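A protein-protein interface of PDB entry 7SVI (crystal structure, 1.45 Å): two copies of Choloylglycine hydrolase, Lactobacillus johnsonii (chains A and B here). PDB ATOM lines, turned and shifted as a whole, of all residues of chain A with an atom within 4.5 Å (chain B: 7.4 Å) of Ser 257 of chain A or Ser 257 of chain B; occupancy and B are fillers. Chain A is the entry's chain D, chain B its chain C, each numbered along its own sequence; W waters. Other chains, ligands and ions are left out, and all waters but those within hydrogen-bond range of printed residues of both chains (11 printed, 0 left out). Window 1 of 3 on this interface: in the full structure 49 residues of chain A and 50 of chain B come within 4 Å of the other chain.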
ATOM      1  N   LYS A 230      26.079  28.354 -16.557  1.00  0.00           N
ATOM      2  CA  LYS A 230      25.190  27.325 -17.081  1.00  0.00           C
ATOM      3  C   LYS A 230      24.255  26.788 -16.001  1.00  0.00           C
ATOM      4  O   LYS A 230      23.046  26.662 -16.235  1.00  0.00           O
ATOM      5  CB  LYS A 230      25.973  26.200 -17.757  1.00  0.00           C
ATOM      6  CG  LYS A 230      25.051  25.119 -18.313  1.00  0.00           C
ATOM      7  CD  LYS A 230      25.754  24.223 -19.323  1.00  0.00           C
ATOM      8  CE  LYS A 230      24.846  23.024 -19.659  1.00  0.00           C
ATOM      9  NZ  LYS A 230      25.416  22.137 -20.727  1.00  0.00           N
ATOM     10  N   LEU A 234      20.233  27.038 -16.254  1.00  0.00           N
ATOM     11  CA  LEU A 234      19.402  25.838 -16.252  1.00  0.00           C
ATOM     12  C   LEU A 234      18.399  25.876 -15.112  1.00  0.00           C
ATOM     13  O   LEU A 234      17.217  25.572 -15.307  1.00  0.00           O
ATOM     14  CB  LEU A 234      20.271  24.587 -16.157  1.00  0.00           C
ATOM     15  CG  LEU A 234      21.178  24.294 -17.352  1.00  0.00           C
ATOM     16  CD1 LEU A 234      21.944  23.016 -17.063  1.00  0.00           C
ATOM     17  CD2 LEU A 234      20.388  24.194 -18.663  1.00  0.00           C
ATOM     18  N   ASN A 253      19.321  15.904 -13.161  1.00  0.00           N
ATOM     19  CA  ASN A 253      19.447  16.350 -14.551  1.00  0.00           C
ATOM     20  C   ASN A 253      20.314  17.599 -14.639  1.00  0.00           C
ATOM     21  O   ASN A 253      21.203  17.695 -15.496  1.00  0.00           O
ATOM     22  CB  ASN A 253      18.072  16.632 -15.160  1.00  0.00           C
ATOM     23  CG  ASN A 253      17.229  15.383 -15.322  1.00  0.00           C
ATOM     24  OD1 ASN A 253      17.760  14.288 -15.459  1.00  0.00           O
ATOM     25  ND2 ASN A 253      15.912  15.550 -15.301  1.00  0.00           N
ATOM     26  N   ILE A 254      20.077  18.564 -13.745  1.00  0.00           N
ATOM     27  CA  ILE A 254      20.828  19.816 -13.789  1.00  0.00           C
ATOM     28  C   ILE A 254      22.281  19.583 -13.393  1.00  0.00           C
ATOM     29  O   ILE A 254      23.208  20.001 -14.098  1.00  0.00           O
ATOM     30  CB  ILE A 254      20.164  20.872 -12.895  1.00  0.00           C
ATOM     31  CG1 ILE A 254      18.786  21.256 -13.438  1.00  0.00           C
ATOM     32  CG2 ILE A 254      21.087  22.087 -12.757  1.00  0.00           C
ATOM     33  CD1 ILE A 254      17.931  22.003 -12.406  1.00  0.00           C
ATOM     34  N   LEU A 255      22.508  18.925 -12.251  1.00  0.00           N
ATOM     35  CA  LEU A 255      23.881  18.750 -11.796  1.00  0.00           C
ATOM     36  C   LEU A 255      24.694  17.836 -12.710  1.00  0.00           C
ATOM     37  O   LEU A 255      25.896  18.051 -12.889  1.00  0.00           O
ATOM     38  CB  LEU A 255      23.914  18.266 -10.344  1.00  0.00           C
ATOM     39  CG  LEU A 255      23.678  19.370  -9.308  1.00  0.00           C
ATOM     40  CD1 LEU A 255      24.157  18.887  -7.970  1.00  0.00           C
ATOM     41  CD2 LEU A 255      24.393  20.665  -9.685  1.00  0.00           C
ATOM     42  N   LYS A 256      24.082  16.806 -13.304  1.00  0.00           N
ATOM     43  CA  LYS A 256      24.871  15.978 -14.213  1.00  0.00           C
ATOM     44  C   LYS A 256      25.202  16.725 -15.499  1.00  0.00           C
ATOM     45  O   LYS A 256      26.205  16.413 -16.151  1.00  0.00           O
ATOM     46  CB  LYS A 256      24.163  14.652 -14.510  1.00  0.00           C
ATOM     47  CG  LYS A 256      24.079  13.716 -13.305  1.00  0.00           C
ATOM     48  CD  LYS A 256      25.448  13.472 -12.705  1.00  0.00           C
ATOM     49  CE  LYS A 256      25.445  12.298 -11.742  1.00  0.00           C
ATOM     50  NZ  LYS A 256      26.778  12.059 -11.165  1.00  0.00           N
ATOM     51  N   SER A 257      24.380  17.708 -15.867  1.00  0.00           N
ATOM     52  CA  SER A 257      24.666  18.524 -17.044  1.00  0.00           C
ATOM     53  C   SER A 257      25.947  19.324 -16.856  1.00  0.00           C
ATOM     54  O   SER A 257      26.724  19.500 -17.804  1.00  0.00           O
ATOM     55  CB  SER A 257      23.486  19.455 -17.326  1.00  0.00           C
ATOM     56  OG  SER A 257      23.783  20.407 -18.350  1.00  0.00           O
ATOM     57  N   VAL A 258      26.185  19.819 -15.640  1.00  0.00           N
ATOM     58  CA  VAL A 258      27.366  20.632 -15.354  1.00  0.00           C
ATOM     59  C   VAL A 258      28.450  19.839 -14.618  1.00  0.00           C
ATOM     60  O   VAL A 258      29.354  20.422 -14.017  1.00  0.00           O
ATOM     61  CB  VAL A 258      27.013  21.950 -14.640  1.00  0.00           C
ATOM     62  CG1 VAL A 258      26.133  22.818 -15.533  1.00  0.00           C
ATOM     63  CG2 VAL A 258      26.319  21.684 -13.306  1.00  0.00           C
ATOM     64  N   ALA A 259      28.393  18.512 -14.672  1.00  0.00           N
ATOM     65  CA  ALA A 259      29.426  17.705 -14.050  1.00  0.00           C
ATOM     66  C   ALA A 259      30.766  17.917 -14.752  1.00  0.00           C
ATOM     67  O   ALA A 259      30.828  18.272 -15.937  1.00  0.00           O
ATOM     68  CB  ALA A 259      29.031  16.227 -14.108  1.00  0.00           C
ATOM     69  N   ILE A 261      33.807  16.087 -16.175  1.00  0.00           N
ATOM     70  CA  ILE A 261      33.850  14.726 -16.705  1.00  0.00           C
ATOM     71  C   ILE A 261      35.273  14.184 -16.662  1.00  0.00           C
ATOM     72  O   ILE A 261      36.216  14.842 -17.119  1.00  0.00           O
ATOM     73  CB  ILE A 261      33.276  14.681 -18.131  1.00  0.00           C
ATOM     74  CG1 ILE A 261      31.847  15.219 -18.135  1.00  0.00           C
ATOM     75  CG2 ILE A 261      33.304  13.254 -18.670  1.00  0.00           C
ATOM     76  CD1 ILE A 261      30.917  14.527 -17.148  1.00  0.00           C
ATOM     77  N   ASN B  19      20.683   9.417 -25.855  1.00  0.00           N
ATOM     78  CA  ASN B  19      19.629  10.290 -25.356  1.00  0.00           C
ATOM     79  C   ASN B  19      18.602  10.461 -26.463  1.00  0.00           C
ATOM     80  O   ASN B  19      18.966  10.678 -27.624  1.00  0.00           O
ATOM     81  CB  ASN B  19      20.170  11.698 -25.074  1.00  0.00           C
ATOM     82  CG  ASN B  19      21.136  11.759 -23.907  1.00  0.00           C
ATOM     83  OD1 ASN B  19      21.105  10.928 -22.992  1.00  0.00           O
ATOM     84  ND2 ASN B  19      21.997  12.787 -23.924  1.00  0.00           N
ATOM     85  N   LEU B 218      34.769  25.229 -25.223  1.00  0.00           N
ATOM     86  CA  LEU B 218      33.899  24.058 -25.386  1.00  0.00           C
ATOM     87  C   LEU B 218      32.452  24.508 -25.262  1.00  0.00           C
ATOM     88  O   LEU B 218      32.093  25.101 -24.241  1.00  0.00           O
ATOM     89  CB  LEU B 218      34.215  23.035 -24.308  1.00  0.00           C
ATOM     90  CG  LEU B 218      33.549  21.655 -24.423  1.00  0.00           C
ATOM     91  CD1 LEU B 218      34.067  20.877 -25.642  1.00  0.00           C
ATOM     92  CD2 LEU B 218      33.781  20.871 -23.135  1.00  0.00           C
ATOM     93  N   GLY B 220      28.416  24.545 -24.591  1.00  0.00           N
ATOM     94  CA  GLY B 220      27.536  23.842 -23.668  1.00  0.00           C
ATOM     95  C   GLY B 220      26.059  23.927 -23.987  1.00  0.00           C
ATOM     96  O   GLY B 220      25.224  23.467 -23.202  1.00  0.00           O
ATOM     97  N   ARG B 227      26.738  19.841 -29.291  1.00  0.00           N
ATOM     98  CA  ARG B 227      26.735  18.572 -28.571  1.00  0.00           C
ATOM     99  C   ARG B 227      27.646  17.544 -29.237  1.00  0.00           C
ATOM    100  O   ARG B 227      28.270  16.738 -28.543  1.00  0.00           O
ATOM    101  CB  ARG B 227      25.308  18.046 -28.415  1.00  0.00           C
ATOM    102  CG  ARG B 227      24.472  18.808 -27.385  1.00  0.00           C
ATOM    103  CD  ARG B 227      23.044  18.250 -27.290  1.00  0.00           C
ATOM    104  NE  ARG B 227      22.237  18.495 -28.486  1.00  0.00           N
ATOM    105  CZ  ARG B 227      22.007  17.576 -29.435  1.00  0.00           C
ATOM    106  NH1 ARG B 227      22.513  16.356 -29.310  1.00  0.00           N
ATOM    107  NH2 ARG B 227      21.268  17.871 -30.494  1.00  0.00           N
ATOM    108  N   LYS B 230      31.254  18.387 -28.073  1.00  0.00           N
ATOM    109  CA  LYS B 230      31.492  18.061 -26.672  1.00  0.00           C
ATOM    110  C   LYS B 230      31.449  16.558 -26.431  1.00  0.00           C
ATOM    111  O   LYS B 230      32.299  16.021 -25.716  1.00  0.00           O
ATOM    112  CB  LYS B 230      30.503  18.795 -25.773  1.00  0.00           C
ATOM    113  CG  LYS B 230      30.729  18.487 -24.300  1.00  0.00           C
ATOM    114  CD  LYS B 230      30.068  19.487 -23.355  1.00  0.00           C
ATOM    115  CE  LYS B 230      30.254  19.016 -21.915  1.00  0.00           C
ATOM    116  NZ  LYS B 230      29.642  19.958 -20.910  1.00  0.00           N
ATOM    117  N   ALA B 231      30.479  15.859 -27.033  1.00  0.00           N
ATOM    118  CA  ALA B 231      30.406  14.414 -26.845  1.00  0.00           C
ATOM    119  C   ALA B 231      31.641  13.721 -27.410  1.00  0.00           C
ATOM    120  O   ALA B 231      32.192  12.816 -26.780  1.00  0.00           O
ATOM    121  CB  ALA B 231      29.129  13.851 -27.472  1.00  0.00           C
ATOM    122  N   LEU B 234      34.561  14.489 -24.966  1.00  0.00           N
ATOM    123  CA  LEU B 234      34.481  13.724 -23.725  1.00  0.00           C
ATOM    124  C   LEU B 234      34.812  12.261 -23.962  1.00  0.00           C
ATOM    125  O   LEU B 234      35.563  11.657 -23.196  1.00  0.00           O
ATOM    126  CB  LEU B 234      33.088  13.847 -23.113  1.00  0.00           C
ATOM    127  CG  LEU B 234      32.700  15.255 -22.668  1.00  0.00           C
ATOM    128  CD1 LEU B 234      31.313  15.245 -22.073  1.00  0.00           C
ATOM    129  CD2 LEU B 234      33.714  15.817 -21.696  1.00  0.00           C
ATOM    130  N   PHE B 251      29.295   5.726 -19.189  1.00  0.00           N
ATOM    131  CA  PHE B 251      28.373   5.992 -20.288  1.00  0.00           C
ATOM    132  C   PHE B 251      27.344   7.052 -19.904  1.00  0.00           C
ATOM    133  O   PHE B 251      27.136   8.032 -20.631  1.00  0.00           O
ATOM    134  CB  PHE B 251      27.692   4.676 -20.686  1.00  0.00           C
ATOM    135  CG  PHE B 251      26.759   4.807 -21.851  1.00  0.00           C
ATOM    136  CD1 PHE B 251      25.457   5.251 -21.673  1.00  0.00           C
ATOM    137  CD2 PHE B 251      27.199   4.512 -23.137  1.00  0.00           C
ATOM    138  CE1 PHE B 251      24.600   5.390 -22.754  1.00  0.00           C
ATOM    139  CE2 PHE B 251      26.353   4.645 -24.223  1.00  0.00           C
ATOM    140  CZ  PHE B 251      25.053   5.083 -24.037  1.00  0.00           C
ATOM    141  N   PHE B 252      26.671   6.861 -18.762  1.00  0.00           N
ATOM    142  CA  PHE B 252      25.680   7.842 -18.331  1.00  0.00           C
ATOM    143  C   PHE B 252      26.325   9.173 -17.959  1.00  0.00           C
ATOM    144  O   PHE B 252      25.697  10.221 -18.131  1.00  0.00           O
ATOM    145  CB  PHE B 252      24.841   7.300 -17.168  1.00  0.00           C
ATOM    146  CG  PHE B 252      23.677   6.457 -17.611  1.00  0.00           C
ATOM    147  CD1 PHE B 252      23.867   5.134 -17.983  1.00  0.00           C
ATOM    148  CD2 PHE B 252      22.406   6.989 -17.685  1.00  0.00           C
ATOM    149  CE1 PHE B 252      22.798   4.361 -18.401  1.00  0.00           C
ATOM    150  CE2 PHE B 252      21.337   6.225 -18.098  1.00  0.00           C
ATOM    151  CZ  PHE B 252      21.535   4.904 -18.473  1.00  0.00           C
ATOM    152  N   ASN B 253      27.567   9.154 -17.468  1.00  0.00           N
ATOM    153  CA  ASN B 253      28.249  10.415 -17.171  1.00  0.00           C
ATOM    154  C   ASN B 253      28.369  11.266 -18.431  1.00  0.00           C
ATOM    155  O   ASN B 253      28.079  12.469 -18.416  1.00  0.00           O
ATOM    156  CB  ASN B 253      29.640  10.148 -16.599  1.00  0.00           C
ATOM    157  CG  ASN B 253      29.601   9.543 -15.203  1.00  0.00           C
ATOM    158  OD1 ASN B 253      28.634   9.736 -14.450  1.00  0.00           O
ATOM    159  ND2 ASN B 253      30.659   8.825 -14.844  1.00  0.00           N
ATOM    160  N   ILE B 254      28.801  10.653 -19.536  1.00  0.00           N
ATOM    161  CA  ILE B 254      28.974  11.397 -20.783  1.00  0.00           C
ATOM    162  C   ILE B 254      27.626  11.859 -21.327  1.00  0.00           C
ATOM    163  O   ILE B 254      27.459  13.022 -21.713  1.00  0.00           O
ATOM    164  CB  ILE B 254      29.737  10.547 -21.815  1.00  0.00           C
ATOM    165  CG1 ILE B 254      31.166  10.241 -21.334  1.00  0.00           C
ATOM    166  CG2 ILE B 254      29.736  11.237 -23.178  1.00  0.00           C
ATOM    167  CD1 ILE B 254      31.857   9.113 -22.114  1.00  0.00           C
ATOM    168  N   LEU B 255      26.654  10.943 -21.428  1.00  0.00           N
ATOM    169  CA  LEU B 255      25.393  11.318 -22.062  1.00  0.00           C
ATOM    170  C   LEU B 255      24.609  12.322 -21.225  1.00  0.00           C
ATOM    171  O   LEU B 255      23.954  13.214 -21.781  1.00  0.00           O
ATOM    172  CB  LEU B 255      24.555  10.081 -22.409  1.00  0.00           C
ATOM    173  CG  LEU B 255      24.970   9.382 -23.707  1.00  0.00           C
ATOM    174  CD1 LEU B 255      23.869   8.426 -24.130  1.00  0.00           C
ATOM    175  CD2 LEU B 255      25.260  10.381 -24.802  1.00  0.00           C
ATOM    176  N   LYS B 256      24.665  12.206 -19.889  1.00  0.00           N
ATOM    177  CA  LYS B 256      23.986  13.206 -19.067  1.00  0.00           C
ATOM    178  C   LYS B 256      24.684  14.564 -19.137  1.00  0.00           C
ATOM    179  O   LYS B 256      24.027  15.600 -18.986  1.00  0.00           O
ATOM    180  CB  LYS B 256      23.824  12.719 -17.624  1.00  0.00           C
ATOM    181  CG  LYS B 256      22.868  11.524 -17.496  1.00  0.00           C
ATOM    182  CD  LYS B 256      21.517  11.817 -18.125  1.00  0.00           C
ATOM    183  CE  LYS B 256      20.439  10.840 -17.639  1.00  0.00           C
ATOM    184  NZ  LYS B 256      19.115  11.117 -18.273  1.00  0.00           N
ATOM    185  N   SER B 257      25.992  14.575 -19.408  1.00  0.00           N
ATOM    186  CA  SER B 257      26.691  15.846 -19.594  1.00  0.00           C
ATOM    187  C   SER B 257      26.141  16.613 -20.791  1.00  0.00           C
ATOM    188  O   SER B 257      26.026  17.842 -20.749  1.00  0.00           O
ATOM    189  CB  SER B 257      28.191  15.601 -19.740  1.00  0.00           C
ATOM    190  OG  SER B 257      28.874  16.789 -20.103  1.00  0.00           O
ATOM    191  N   VAL B 258      25.794  15.907 -21.868  1.00  0.00           N
ATOM    192  CA  VAL B 258      25.319  16.539 -23.100  1.00  0.00           C
ATOM    193  C   VAL B 258      23.798  16.428 -23.255  1.00  0.00           C
ATOM    194  O   VAL B 258      23.272  16.609 -24.354  1.00  0.00           O
ATOM    195  CB  VAL B 258      26.062  16.031 -24.345  1.00  0.00           C
ATOM    196  CG1 VAL B 258      27.525  16.442 -24.291  1.00  0.00           C
ATOM    197  CG2 VAL B 258      25.939  14.490 -24.479  1.00  0.00           C
ATOM    198  N   ALA B 259      23.082  16.139 -22.171  1.00  0.00           N
ATOM    199  CA  ALA B 259      21.631  16.094 -22.242  1.00  0.00           C
ATOM    200  C   ALA B 259      21.062  17.466 -22.578  1.00  0.00           C
ATOM    201  O   ALA B 259      21.668  18.509 -22.300  1.00  0.00           O
ATOM    202  CB  ALA B 259      21.042  15.607 -20.911  1.00  0.00           C
ATOM    203  N   MET B 260      19.876  17.457 -23.177  1.00  0.00           N
ATOM    204  CA  MET B 260      19.124  18.665 -23.495  1.00  0.00           C
ATOM    205  C   MET B 260      18.163  18.911 -22.339  1.00  0.00           C
ATOM    206  O   MET B 260      17.245  18.128 -22.114  1.00  0.00           O
ATOM    207  CB  MET B 260      18.368  18.441 -24.807  1.00  0.00           C
ATOM    208  CG  MET B 260      17.651  19.670 -25.326  1.00  0.00           C
ATOM    209  SD  MET B 260      16.824  19.374 -26.903  1.00  0.00           S
ATOM    210  CE  MET B 260      18.209  18.872 -27.919  1.00  0.00           C
ATOM    211  N   ILE B 261      18.379  19.983 -21.586  1.00  0.00           N
ATOM    212  CA  ILE B 261      17.760  20.132 -20.268  1.00  0.00           C
ATOM    213  C   ILE B 261      16.409  20.835 -20.383  1.00  0.00           C
ATOM    214  O   ILE B 261      16.282  21.871 -21.043  1.00  0.00           O
ATOM    215  CB  ILE B 261      18.712  20.881 -19.319  1.00  0.00           C
ATOM    216  CG1 ILE B 261      20.061  20.162 -19.235  1.00  0.00           C
ATOM    217  CG2 ILE B 261      18.108  21.036 -17.916  1.00  0.00           C
ATOM    218  CD1 ILE B 261      19.981  18.692 -18.810  1.00  0.00           C
HETATM  219  O   HOH W   1      27.036  20.059 -21.931  1.00  0.00           O
HETATM  220  O   HOH W   2      21.535  15.543 -17.424  1.00  0.00           O
HETATM  221  O   HOH W   3      16.968  11.857 -16.524  1.00  0.00           O
HETATM  222  O   HOH W   4      22.734  22.403 -22.349  1.00  0.00           O
HETATM  223  O   HOH W   5      23.808  19.500 -20.911  1.00  0.00           O
HETATM  224  O   HOH W   6      28.588  12.406 -13.746  1.00  0.00           O
HETATM  225  O   HOH W   7      29.255  18.671 -18.287  1.00  0.00           O
HETATM  226  O   HOH W   8      27.428  13.759 -15.922  1.00  0.00           O
HETATM  227  O   HOH W   9      28.202   9.633 -11.740  1.00  0.00           O
HETATM  228  O   HOH W  10      19.139  14.289 -17.951  1.00  0.00           O
HETATM  229  O   HOH W  11      27.770  21.527 -19.300  1.00  0.00           O
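The side-chain amino group (NZ) of Lys 230 of chain B sits close to the side-chain hydroxyl (OG) of Ser 257 of chain B (3.4 Å). NZ of Lys 230 of chain A sits close to OG of Ser 257 of chain A (3.4 Å).
Of the 10 printed residues of chain A, 6 touch a printed residue of chain B. Hydrophobic or aromatic side chains of chain A that line the printed part of chain B: Leu 234 and Ile 261. Printed residues of chain B that touch a printed residue of chain A: Gly 220, Leu 234, Asn 253, Lys 256, Ser 257 and Ile 261. Hydrophobic or aromatic side chains of chain B within 4 Å of the printed part of chain A: Leu 234 and Ile 261. Among the printed residues, 11 pairs touch across the chains. Among the printed residues, no Asp or Glu carboxylate lies within 4 Å of a Lys or Arg side-chain nitrogen of the other chain.
O of Ser 257 of chain A sits close to O of Ser 257 of chain B. NZ of Lys 230 of chain A is in hydrogen-bond range of O of Gly 220 of chain B (2.8 Å).
Asn 253 of chain A touches Ile 261 of chain B, and with the chains exchanged Ile 261 of chain A touches Asn 253 of chain B. Lys 256 of chain B touches its own counterpart, Lys 256 of chain A. Lys 256 of chain A touches Ser 257 of chain B, and with the chains exchanged Ser 257 of chain A touches Lys 256 of chain B. Ser 257 of chain A touches its own counterpart, Ser 257 of chain B.
Printed residues of chain B within 4 Å of Lys 230 of chain A: Gly 220. Printed residues of chain B within 4 Å of Asn 253 of chain A: Ile 261 (3.7 Å). Of the printed residues of chain B, Lys 256 of chain A touches Lys 256 and Ser 257. Ser 257 of chain A touches three residues of chain B. Printed residues of chain B within 4 Å of Ile 261 of chain A: Leu 234, Asn 253 and Ser 257. Printed residues of chain A within 4 Å of Gly 220 of chain B: Lys 230. Lys 230 of chain B touches none of the printed residues of chain A. Leu 255 of chain B touches none of the printed residues of chain A. Of the printed residues of chain A, Ser 257 of chain B touches Lys 256, Ser 257 and Ile 261. The nearest residue of chain A that does not touch Ser 257 of chain B is Lys 230 of chain A (4.3 Å). The nearest printed residue of chain B that does not touch Ile 261 of chain A is Ile 254 of chain B (4.6 Å).
Leu 234 of chain A touches Ile 261 of chain B. CD1 of Ile 261 of chain B touches O of Asn 253 of chain A, 3.7 Å away. Lys 256 of chain B touches Lys 256 of chain A. Lys 256 of chain A touches Ser 257 of chain B. CA of Ser 257 of chain A touches O of Lys 256 of chain B, at 3.6 Å. Ser 257 of chain A touches Ile 261 of chain B (OG to CG1, 3.8 Å). Ile 261 of chain A touches Leu 234 of chain B (CB to CD2, 3.8 Å). CD1 of Ile 261 of chain A touches O of Asn 253 of chain B (3.7 Å). Ile 261 of chain A touches Ser 257 of chain B.
Water W1 lies within hydrogen-bond range of O of Ser 257 of chain B, NZ of Lys 230 of chain B and NZ of Lys 230 of chain A. Water W5 lies within hydrogen-bond range of the side-chain hydroxyl of Ser 257 of chain A (2.7 Å), the backbone carbonyl oxygen of Ala 259 of chain B (2.7 Å), the backbone carbonyl oxygen of Ser 257 of chain B (2.8 Å) and the side-chain amino group of Lys 230 of chain A (3.1 Å). Water W3 lies within hydrogen-bond range of OD1 of Asn 253 of chain A (2.8 Å) and NZ of Lys 256 of chain B (2.9 Å). Water W4 bridges the backbone carbonyl oxygen (O) of Gly 220 of chain B (2.8 Å) and the side-chain amino group (NZ) of Lys 230 of chain A (3.1 Å). Water W8 bridges the backbone carbonyl oxygen (O) of Asn 253 of chain B and the backbone carbonyl oxygen (O) of Lys 256 of chain A. Water W2 bridges O of Asn 253 of chain A (2.9 Å) and O of Lys 256 of chain B (2.9 Å).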
